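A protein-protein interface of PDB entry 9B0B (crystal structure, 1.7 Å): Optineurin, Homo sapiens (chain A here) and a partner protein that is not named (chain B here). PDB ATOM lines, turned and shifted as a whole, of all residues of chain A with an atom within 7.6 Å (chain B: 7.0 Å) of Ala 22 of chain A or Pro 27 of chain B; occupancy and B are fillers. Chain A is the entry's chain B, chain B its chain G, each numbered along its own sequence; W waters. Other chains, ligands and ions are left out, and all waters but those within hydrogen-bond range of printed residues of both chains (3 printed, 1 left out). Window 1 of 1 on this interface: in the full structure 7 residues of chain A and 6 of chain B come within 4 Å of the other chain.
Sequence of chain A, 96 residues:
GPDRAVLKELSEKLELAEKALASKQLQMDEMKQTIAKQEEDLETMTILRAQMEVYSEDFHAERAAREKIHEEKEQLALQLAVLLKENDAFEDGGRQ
NH1 of Arg 28 of chain B lies within salt-bridge range of OE2 of Glu 18 of chain A.
The side-chain carboxylate (OD2) of Asp 29 of chain A is in salt-bridge range of the guanidinium group (NH1) of Arg 26 of chain B, 2.9 Å away.
The side-chain amide nitrogen (NE2) of Gln 25 of chain A sits close to the guanidinium group (NH1) of Arg 26 of chain B.
The backbone NH of Arg 26 of chain B sits close to the side-chain sulfur of Cys 24 of chain B (3.7 Å).
O of Lys 19 of chain A lies within hydrogen-bond range of OG of Ser 23 of chain A (3.0 Å).
The backbone carbonyl oxygen (O) of Val 19 of chain B is in hydrogen-bond range of the backbone NH (N) of Arg 28 of chain B, 3.3 Å away.
The guanidinium group (NH2) of Arg 26 of chain B is in salt-bridge range of the chain-end carboxylate (O) of Ala 30 of chain B (3.1 Å).
The side-chain amide nitrogen of Gln 25 of chain A sits at hydrogen-bond distance from the side-chain carboxylate of Asp 29 of chain A, 3.2 Å away.
N of Cys 21 of chain B lies within hydrogen-bond range of O of Arg 26 of chain B, at 2.8 Å.
Among the printed residues, pairs that only touch across the chains: Glu 18 of chain A with Leu 29 of chain B (3.9 Å), Lys 19 of chain A with Leu 29 of chain B (3.8 Å), Leu 21 of chain A with Leu 20 of chain B (3.9 Å), Leu 21 of chain A with Pro 27 of chain B (3.6 Å), Ala 22 of chain A with Pro 27 of chain B (3.9 Å), Ala 22 of chain A with Leu 29 of chain B (3.4 Å), Ala 22 of chain A with Ala 30 of chain B (3.6 Å), Gln 25 of chain A with Pro 27 of chain B (3.4 Å) and Gln 25 of chain A with Ala 30 of chain B (3.9 Å).
Printed residues of chain B within 4 Å of Ala 22 of chain A: Pro 27, Leu 29 and Ala 30.
Of the printed residues of chain B, Asp 29 of chain A touches Arg 26.
Printed residues of chain A within 4 Å of Leu 20 of chain B: Leu 21 (3.9 Å).
Printed residues of chain B within 4 Å of Glu 18 of chain A: Arg 28 and Leu 29.
Of the printed residues of chain B, Leu 21 of chain A touches Leu 20 (3.9 Å) and Pro 27 (3.6 Å).
Printed residues of chain B within 4 Å of Lys 19 of chain A: Leu 29.
The nearest residue of chain B that does not touch Ala 22 of chain A is Arg 28 of chain B (5.5 Å).
The nearest residue of chain A that does not touch Pro 27 of chain B is Glu 18 of chain A (5.0 Å).
The nearest printed residue of chain B that does not touch Lys 19 of chain A is Arg 28 of chain B (6.7 Å).
Of the 13 printed residues of chain B, 6 touch a printed residue of chain A.
Hydrophobic or aromatic side chains of chain B within 4 Å of the printed part of chain A: Leu 20, Pro 27, Leu 29 and Ala 30.
Of the 14 printed residues of chain A, 6 touch a printed residue of chain B.
Among the printed residues, 12 pairs touch across the chains.
Water W3 lies within hydrogen-bond range of OE1 of Glu 18 of chain A (2.6 Å), O of Val 19 of chain B (2.7 Å) and N of Arg 28 of chain B (3.4 Å).
Water W1 bridges OE1 of Glu 18 of chain A (2.7 Å) and NE of Arg 28 of chain B (3.2 Å).
Water W2 lies within hydrogen-bond range of the backbone NH of Leu 29 of chain B (2.8 Å), the backbone carbonyl oxygen of Glu 18 of chain A (2.8 Å) and the backbone NH of Arg 28 of chain B (3.3 Å).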
ATOM      1  N   LEU A  16      -6.670  20.396  -1.962  1.00  0.00           N
ATOM      2  CA  LEU A  16      -5.679  20.059  -2.979  1.00  0.00           C
ATOM      3  C   LEU A  16      -6.296  19.191  -4.087  1.00  0.00           C
ATOM      4  O   LEU A  16      -5.915  19.303  -5.272  1.00  0.00           O
ATOM      5  CB  LEU A  16      -4.476  19.355  -2.352  1.00  0.00           C
ATOM      6  CG  LEU A  16      -3.560  20.282  -1.507  1.00  0.00           C
ATOM      7  CD1 LEU A  16      -2.390  19.454  -0.939  1.00  0.00           C
ATOM      8  CD2 LEU A  16      -2.966  21.420  -2.335  1.00  0.00           C
ATOM      9  N   ALA A  17      -7.168  18.255  -3.718  1.00  0.00           N
ATOM     10  CA  ALA A  17      -7.795  17.447  -4.765  1.00  0.00           C
ATOM     11  C   ALA A  17      -8.620  18.340  -5.685  1.00  0.00           C
ATOM     12  O   ALA A  17      -8.600  18.159  -6.902  1.00  0.00           O
ATOM     13  CB  ALA A  17      -8.682  16.345  -4.176  1.00  0.00           C
ATOM     14  N   GLU A  18      -9.330  19.321  -5.120  1.00  0.00           N
ATOM     15  CA  GLU A  18     -10.141  20.201  -5.973  1.00  0.00           C
ATOM     16  C   GLU A  18      -9.270  21.102  -6.835  1.00  0.00           C
ATOM     17  O   GLU A  18      -9.630  21.402  -7.973  1.00  0.00           O
ATOM     18  CB  GLU A  18     -11.127  21.013  -5.121  1.00  0.00           C
ATOM     19  CG  GLU A  18     -12.206  20.141  -4.516  1.00  0.00           C
ATOM     20  CD  GLU A  18     -13.363  20.998  -3.986  1.00  0.00           C
ATOM     21  OE1 GLU A  18     -14.331  21.247  -4.763  1.00  0.00           O
ATOM     22  OE2 GLU A  18     -13.242  21.481  -2.857  1.00  0.00           O
ATOM     23  N   LYS A  19      -8.096  21.535  -6.324  1.00  0.00           N
ATOM     24  CA  LYS A  19      -7.199  22.314  -7.167  1.00  0.00           C
ATOM     25  C   LYS A  19      -6.618  21.480  -8.295  1.00  0.00           C
ATOM     26  O   LYS A  19      -6.524  21.960  -9.424  1.00  0.00           O
ATOM     27  CB  LYS A  19      -6.041  22.915  -6.300  1.00  0.00           C
ATOM     28  CG  LYS A  19      -6.603  24.019  -5.408  1.00  0.00           C
ATOM     29  CD  LYS A  19      -5.557  24.665  -4.513  1.00  0.00           C
ATOM     30  CE  LYS A  19      -4.404  25.186  -5.343  1.00  0.00           C
ATOM     31  NZ  LYS A  19      -4.747  26.508  -5.964  1.00  0.00           N
ATOM     32  N   ALA A  20      -6.255  20.225  -8.019  1.00  0.00           N
ATOM     33  CA  ALA A  20      -5.719  19.365  -9.066  1.00  0.00           C
ATOM     34  C   ALA A  20      -6.805  19.045 -10.078  1.00  0.00           C
ATOM     35  O   ALA A  20      -6.557  19.034 -11.272  1.00  0.00           O
ATOM     36  CB  ALA A  20      -5.179  18.058  -8.488  1.00  0.00           C
ATOM     37  N   LEU A  21      -8.024  18.843  -9.596  1.00  0.00           N
ATOM     38  CA  LEU A  21      -9.145  18.587 -10.503  1.00  0.00           C
ATOM     39  C   LEU A  21      -9.376  19.762 -11.444  1.00  0.00           C
ATOM     40  O   LEU A  21      -9.565  19.597 -12.663  1.00  0.00           O
ATOM     41  CB  LEU A  21     -10.386  18.296  -9.613  1.00  0.00           C
ATOM     42  CG  LEU A  21     -11.606  17.726 -10.286  1.00  0.00           C
ATOM     43  CD1 LEU A  21     -11.406  16.463 -11.144  1.00  0.00           C
ATOM     44  CD2 LEU A  21     -12.657  17.504  -9.116  1.00  0.00           C
ATOM     45  N   ALA A  22      -9.409  20.975 -10.882  1.00  0.00           N
ATOM     46  CA  ALA A  22      -9.595  22.170 -11.699  1.00  0.00           C
ATOM     47  C   ALA A  22      -8.454  22.315 -12.694  1.00  0.00           C
ATOM     48  O   ALA A  22      -8.663  22.667 -13.857  1.00  0.00           O
ATOM     49  CB  ALA A  22      -9.669  23.414 -10.803  1.00  0.00           C
ATOM     50  N   SER A  23      -7.216  22.043 -12.244  1.00  0.00           N
ATOM     51  CA  SER A  23      -6.100  22.113 -13.160  1.00  0.00           C
ATOM     52  C   SER A  23      -6.182  21.077 -14.286  1.00  0.00           C
ATOM     53  O   SER A  23      -5.784  21.381 -15.408  1.00  0.00           O
ATOM     54  CB  SER A  23      -4.794  21.957 -12.359  1.00  0.00           C
ATOM     55  OG  SER A  23      -4.648  23.065 -11.470  1.00  0.00           O
ATOM     56  N   LYS A  24      -6.674  19.860 -14.018  1.00  0.00           N
ATOM     57  CA  LYS A  24      -6.868  18.936 -15.140  1.00  0.00           C
ATOM     58  C   LYS A  24      -7.891  19.502 -16.117  1.00  0.00           C
ATOM     59  O   LYS A  24      -7.756  19.366 -17.327  1.00  0.00           O
ATOM     60  CB  LYS A  24      -7.358  17.573 -14.669  1.00  0.00           C
ATOM     61  CG  LYS A  24      -6.245  16.768 -13.809  1.00  0.00           C
ATOM     62  CD  LYS A  24      -6.638  15.277 -13.641  1.00  0.00           C
ATOM     63  CE  LYS A  24      -5.668  14.482 -12.675  1.00  0.00           C
ATOM     64  NZ  LYS A  24      -4.523  14.159 -13.496  1.00  0.00           N
ATOM     65  N   GLN A  25      -8.948  20.117 -15.587  1.00  0.00           N
ATOM     66  CA  GLN A  25      -9.955  20.668 -16.499  1.00  0.00           C
ATOM     67  C   GLN A  25      -9.332  21.746 -17.379  1.00  0.00           C
ATOM     68  O   GLN A  25      -9.627  21.851 -18.580  1.00  0.00           O
ATOM     69  CB  GLN A  25     -11.124  21.250 -15.674  1.00  0.00           C
ATOM     70  CG  GLN A  25     -12.238  21.825 -16.635  1.00  0.00           C
ATOM     71  CD  GLN A  25     -12.929  20.748 -17.378  1.00  0.00           C
ATOM     72  OE1 GLN A  25     -13.537  19.891 -16.755  1.00  0.00           O
ATOM     73  NE2 GLN A  25     -12.866  20.772 -18.712  1.00  0.00           N
ATOM     74  N   LEU A  26      -8.478  22.576 -16.789  1.00  0.00           N
ATOM     75  CA  LEU A  26      -7.846  23.642 -17.557  1.00  0.00           C
ATOM     76  C   LEU A  26      -6.936  23.048 -18.623  1.00  0.00           C
ATOM     77  O   LEU A  26      -6.857  23.562 -19.745  1.00  0.00           O
ATOM     78  CB  LEU A  26      -7.058  24.573 -16.622  1.00  0.00           C
ATOM     79  CG  LEU A  26      -7.997  25.368 -15.669  1.00  0.00           C
ATOM     80  CD1 LEU A  26      -7.175  26.119 -14.598  1.00  0.00           C
ATOM     81  CD2 LEU A  26      -9.015  26.311 -16.352  1.00  0.00           C
ATOM     82  N   GLN A  27      -6.266  21.946 -18.291  1.00  0.00           N
ATOM     83  CA  GLN A  27      -5.483  21.270 -19.321  1.00  0.00           C
ATOM     84  C   GLN A  27      -6.393  20.752 -20.436  1.00  0.00           C
ATOM     85  O   GLN A  27      -6.037  20.815 -21.620  1.00  0.00           O
ATOM     86  CB  GLN A  27      -4.690  20.112 -18.722  1.00  0.00           C
ATOM     87  CG  GLN A  27      -3.529  20.543 -17.773  1.00  0.00           C
ATOM     88  CD  GLN A  27      -2.897  19.329 -17.114  1.00  0.00           C
ATOM     89  OE1 GLN A  27      -3.587  18.471 -16.514  1.00  0.00           O
ATOM     90  NE2 GLN A  27      -1.580  19.259 -17.166  1.00  0.00           N
ATOM     91  N   MET A  28      -7.532  20.174 -20.062  1.00  0.00           N
ATOM     92  CA  MET A  28      -8.502  19.696 -21.066  1.00  0.00           C
ATOM     93  C   MET A  28      -8.988  20.830 -21.951  1.00  0.00           C
ATOM     94  O   MET A  28      -9.178  20.651 -23.177  1.00  0.00           O
ATOM     95  CB  MET A  28      -9.696  19.041 -20.355  1.00  0.00           C
ATOM     96  CG  MET A  28      -9.272  17.811 -19.650  1.00  0.00           C
ATOM     97  SD  MET A  28     -10.589  17.095 -18.660  1.00  0.00           S
ATOM     98  CE  MET A  28     -11.881  16.919 -19.932  1.00  0.00           C
ATOM     99  N   ASP A  29      -9.224  22.008 -21.346  1.00  0.00           N
ATOM    100  CA  ASP A  29      -9.660  23.139 -22.156  1.00  0.00           C
ATOM    101  C   ASP A  29      -8.622  23.469 -23.222  1.00  0.00           C
ATOM    102  O   ASP A  29      -8.970  23.788 -24.366  1.00  0.00           O
ATOM    103  CB  ASP A  29      -9.885  24.378 -21.307  1.00  0.00           C
ATOM    104  CG  ASP A  29     -11.025  24.213 -20.293  1.00  0.00           C
ATOM    105  OD1 ASP A  29     -10.999  25.032 -19.351  1.00  0.00           O
ATOM    106  OD2 ASP A  29     -11.901  23.297 -20.423  1.00  0.00           O
ATOM    107  N   TRP B   5     -22.272  26.253  -4.099  1.00  0.00           N
ATOM    108  CA  TRP B   5     -21.314  27.014  -4.863  1.00  0.00           C
ATOM    109  C   TRP B   5     -21.823  27.159  -6.288  1.00  0.00           C
ATOM    110  O   TRP B   5     -22.417  26.233  -6.847  1.00  0.00           O
ATOM    111  CB  TRP B   5     -19.927  26.333  -4.907  1.00  0.00           C
ATOM    112  CG  TRP B   5     -19.921  24.907  -5.314  1.00  0.00           C
ATOM    113  CD1 TRP B   5     -20.118  23.807  -4.514  1.00  0.00           C
ATOM    114  CD2 TRP B   5     -19.645  24.396  -6.635  1.00  0.00           C
ATOM    115  NE1 TRP B   5     -20.031  22.642  -5.272  1.00  0.00           N
ATOM    116  CE2 TRP B   5     -19.698  22.985  -6.565  1.00  0.00           C
ATOM    117  CE3 TRP B   5     -19.414  25.010  -7.881  1.00  0.00           C
ATOM    118  CZ2 TRP B   5     -19.491  22.166  -7.694  1.00  0.00           C
ATOM    119  CZ3 TRP B   5     -19.186  24.174  -9.014  1.00  0.00           C
ATOM    120  CH2 TRP B   5     -19.222  22.793  -8.904  1.00  0.00           C
ATOM    121  N   CYS B   7     -21.327  27.422 -10.290  1.00  0.00           N
ATOM    122  CA  CYS B   7     -20.427  27.103 -11.403  1.00  0.00           C
ATOM    123  C   CYS B   7     -20.032  28.387 -12.120  1.00  0.00           C
ATOM    124  O   CYS B   7     -20.894  29.146 -12.561  1.00  0.00           O
ATOM    125  CB  CYS B   7     -21.102  26.144 -12.399  1.00  0.00           C
ATOM    126  SG  CYS B   7     -20.151  25.743 -13.831  1.00  0.00           S
ATOM    127  N   GLN B   8     -18.722  28.617 -12.271  1.00  0.00           N
ATOM    128  CA  GLN B   8     -18.268  29.863 -12.884  1.00  0.00           C
ATOM    129  C   GLN B   8     -18.429  29.874 -14.409  1.00  0.00           C
ATOM    130  O   GLN B   8     -18.190  30.912 -15.028  1.00  0.00           O
ATOM    131  CB  GLN B   8     -16.787  30.105 -12.543  1.00  0.00           C
ATOM    132  CG  GLN B   8     -16.559  30.174 -11.033  1.00  0.00           C
ATOM    133  CD  GLN B   8     -17.258  31.377 -10.450  1.00  0.00           C
ATOM    134  OE1 GLN B   8     -16.928  32.516 -10.773  1.00  0.00           O
ATOM    135  NE2 GLN B   8     -18.260  31.128  -9.590  1.00  0.00           N
ATOM    136  N   VAL B  19     -18.481  18.051  -6.356  1.00  0.00           N
ATOM    137  CA  VAL B  19     -17.174  18.562  -6.775  1.00  0.00           C
ATOM    138  C   VAL B  19     -17.160  18.940  -8.264  1.00  0.00           C
ATOM    139  O   VAL B  19     -16.320  19.765  -8.670  1.00  0.00           O
ATOM    140  CB  VAL B  19     -16.015  17.571  -6.482  1.00  0.00           C
ATOM    141  CG1 VAL B  19     -15.851  17.334  -4.939  1.00  0.00           C
ATOM    142  CG2 VAL B  19     -16.205  16.278  -7.298  1.00  0.00           C
ATOM    143  N   LEU B  20     -18.096  18.422  -9.058  1.00  0.00           N
ATOM    144  CA  LEU B  20     -18.230  18.780 -10.468  1.00  0.00           C
ATOM    145  C   LEU B  20     -19.598  19.449 -10.619  1.00  0.00           C
ATOM    146  O   LEU B  20     -20.560  19.062  -9.951  1.00  0.00           O
ATOM    147  CB  LEU B  20     -18.190  17.557 -11.378  1.00  0.00           C
ATOM    148  CG  LEU B  20     -16.839  16.819 -11.395  1.00  0.00           C
ATOM    149  CD1 LEU B  20     -16.935  15.691 -12.443  1.00  0.00           C
ATOM    150  CD2 LEU B  20     -15.623  17.762 -11.641  1.00  0.00           C
ATOM    151  N   CYS B  21     -19.689  20.410 -11.525  1.00  0.00           N
ATOM    152  CA  CYS B  21     -21.000  21.012 -11.752  1.00  0.00           C
ATOM    153  C   CYS B  21     -21.997  19.958 -12.256  1.00  0.00           C
ATOM    154  O   CYS B  21     -21.698  19.175 -13.148  1.00  0.00           O
ATOM    155  CB  CYS B  21     -20.840  22.135 -12.767  1.00  0.00           C
ATOM    156  SG  CYS B  21     -22.470  23.033 -13.291  1.00  0.00           S
ATOM    157  N   CYS B  24     -22.662  21.053 -16.234  1.00  0.00           N
ATOM    158  CA  CYS B  24     -21.607  21.035 -17.252  1.00  0.00           C
ATOM    159  C   CYS B  24     -20.381  20.167 -16.865  1.00  0.00           C
ATOM    160  O   CYS B  24     -19.416  20.083 -17.635  1.00  0.00           O
ATOM    161  CB  CYS B  24     -21.206  22.485 -17.584  1.00  0.00           C
ATOM    162  SG  CYS B  24     -20.310  23.284 -16.283  1.00  0.00           S
ATOM    163  N   GLU B  25     -20.373  19.623 -15.655  1.00  0.00           N
ATOM    164  CA  GLU B  25     -19.335  18.737 -15.136  1.00  0.00           C
ATOM    165  C   GLU B  25     -17.994  19.435 -14.913  1.00  0.00           C
ATOM    166  O   GLU B  25     -17.000  18.757 -14.776  1.00  0.00           O
ATOM    167  CB  GLU B  25     -19.102  17.523 -16.021  1.00  0.00           C
ATOM    168  CG  GLU B  25     -20.314  16.675 -16.246  1.00  0.00           C
ATOM    169  CD  GLU B  25     -20.030  15.496 -17.196  1.00  0.00           C
ATOM    170  OE1 GLU B  25     -18.904  15.378 -17.772  1.00  0.00           O
ATOM    171  OE2 GLU B  25     -20.956  14.675 -17.336  1.00  0.00           O
ATOM    172  N   ARG B  26     -17.961  20.733 -14.902  1.00  0.00           N
ATOM    173  CA  ARG B  26     -16.668  21.375 -14.647  1.00  0.00           C
ATOM    174  C   ARG B  26     -16.414  21.450 -13.153  1.00  0.00           C
ATOM    175  O   ARG B  26     -17.316  21.698 -12.367  1.00  0.00           O
ATOM    176  CB  ARG B  26     -16.667  22.802 -15.223  1.00  0.00           C
ATOM    177  CG  ARG B  26     -16.638  22.799 -16.849  1.00  0.00           C
ATOM    178  CD  ARG B  26     -16.572  24.248 -17.350  1.00  0.00           C
ATOM    179  NE  ARG B  26     -15.314  24.907 -16.997  1.00  0.00           N
ATOM    180  CZ  ARG B  26     -14.181  24.756 -17.720  1.00  0.00           C
ATOM    181  NH1 ARG B  26     -14.160  23.964 -18.793  1.00  0.00           N
ATOM    182  NH2 ARG B  26     -13.078  25.380 -17.357  1.00  0.00           N
ATOM    183  N   PRO B  27     -15.159  21.315 -12.739  1.00  0.00           N
ATOM    184  CA  PRO B  27     -14.839  21.410 -11.323  1.00  0.00           C
ATOM    185  C   PRO B  27     -15.066  22.791 -10.799  1.00  0.00           C
ATOM    186  O   PRO B  27     -14.942  23.786 -11.512  1.00  0.00           O
ATOM    187  CB  PRO B  27     -13.315  21.077 -11.283  1.00  0.00           C
ATOM    188  CG  PRO B  27     -13.100  20.211 -12.522  1.00  0.00           C
ATOM    189  CD  PRO B  27     -14.041  20.914 -13.599  1.00  0.00           C
ATOM    190  N   ARG B  28     -15.357  22.849  -9.491  1.00  0.00           N
ATOM    191  CA  ARG B  28     -15.664  24.106  -8.835  1.00  0.00           C
ATOM    192  C   ARG B  28     -14.592  25.168  -9.059  1.00  0.00           C
ATOM    193  O   ARG B  28     -14.913  26.352  -9.225  1.00  0.00           O
ATOM    194  CB  ARG B  28     -15.842  23.857  -7.322  1.00  0.00           C
ATOM    195  CG  ARG B  28     -16.059  25.160  -6.535  1.00  0.00           C
ATOM    196  CD  ARG B  28     -16.367  24.837  -5.062  1.00  0.00           C
ATOM    197  NE  ARG B  28     -15.176  24.295  -4.356  1.00  0.00           N
ATOM    198  CZ  ARG B  28     -14.272  25.032  -3.742  1.00  0.00           C
ATOM    199  NH1 ARG B  28     -13.228  24.461  -3.117  1.00  0.00           N
ATOM    200  NH2 ARG B  28     -14.433  26.343  -3.689  1.00  0.00           N
ATOM    201  N   LEU B  29     -13.302  24.797  -9.015  1.00  0.00           N
ATOM    202  CA  LEU B  29     -12.308  25.851  -9.105  1.00  0.00           C
ATOM    203  C   LEU B  29     -11.791  26.046 -10.531  1.00  0.00           C
ATOM    204  O   LEU B  29     -10.767  26.722 -10.713  1.00  0.00           O
ATOM    205  CB  LEU B  29     -11.118  25.611  -8.156  1.00  0.00           C
ATOM    206  CG  LEU B  29     -11.481  25.435  -6.673  1.00  0.00           C
ATOM    207  CD1 LEU B  29     -10.342  24.762  -5.855  1.00  0.00           C
ATOM    208  CD2 LEU B  29     -11.884  26.810  -6.163  1.00  0.00           C
ATOM    209  N   ALA B  30     -12.497  25.514 -11.523  1.00  0.00           N
ATOM    210  CA  ALA B  30     -12.073  25.681 -12.934  1.00  0.00           C
ATOM    211  C   ALA B  30     -12.851  26.799 -13.589  1.00  0.00           C
ATOM    212  O   ALA B  30     -12.645  27.064 -14.777  1.00  0.00           O
ATOM    213  CB  ALA B  30     -12.263  24.419 -13.734  1.00  0.00           C
ATOM    214  OXT ALA B  30     -13.706  27.425 -12.959  1.00  0.00           O
HETATM  215  O   HOH W   1     -16.884  21.625  -4.078  1.00  0.00           O
HETATM  216  O   HOH W   2     -12.307  22.248  -8.378  1.00  0.00           O
HETATM  217  O   HOH W   3     -14.125  20.562  -7.241  1.00  0.00           O
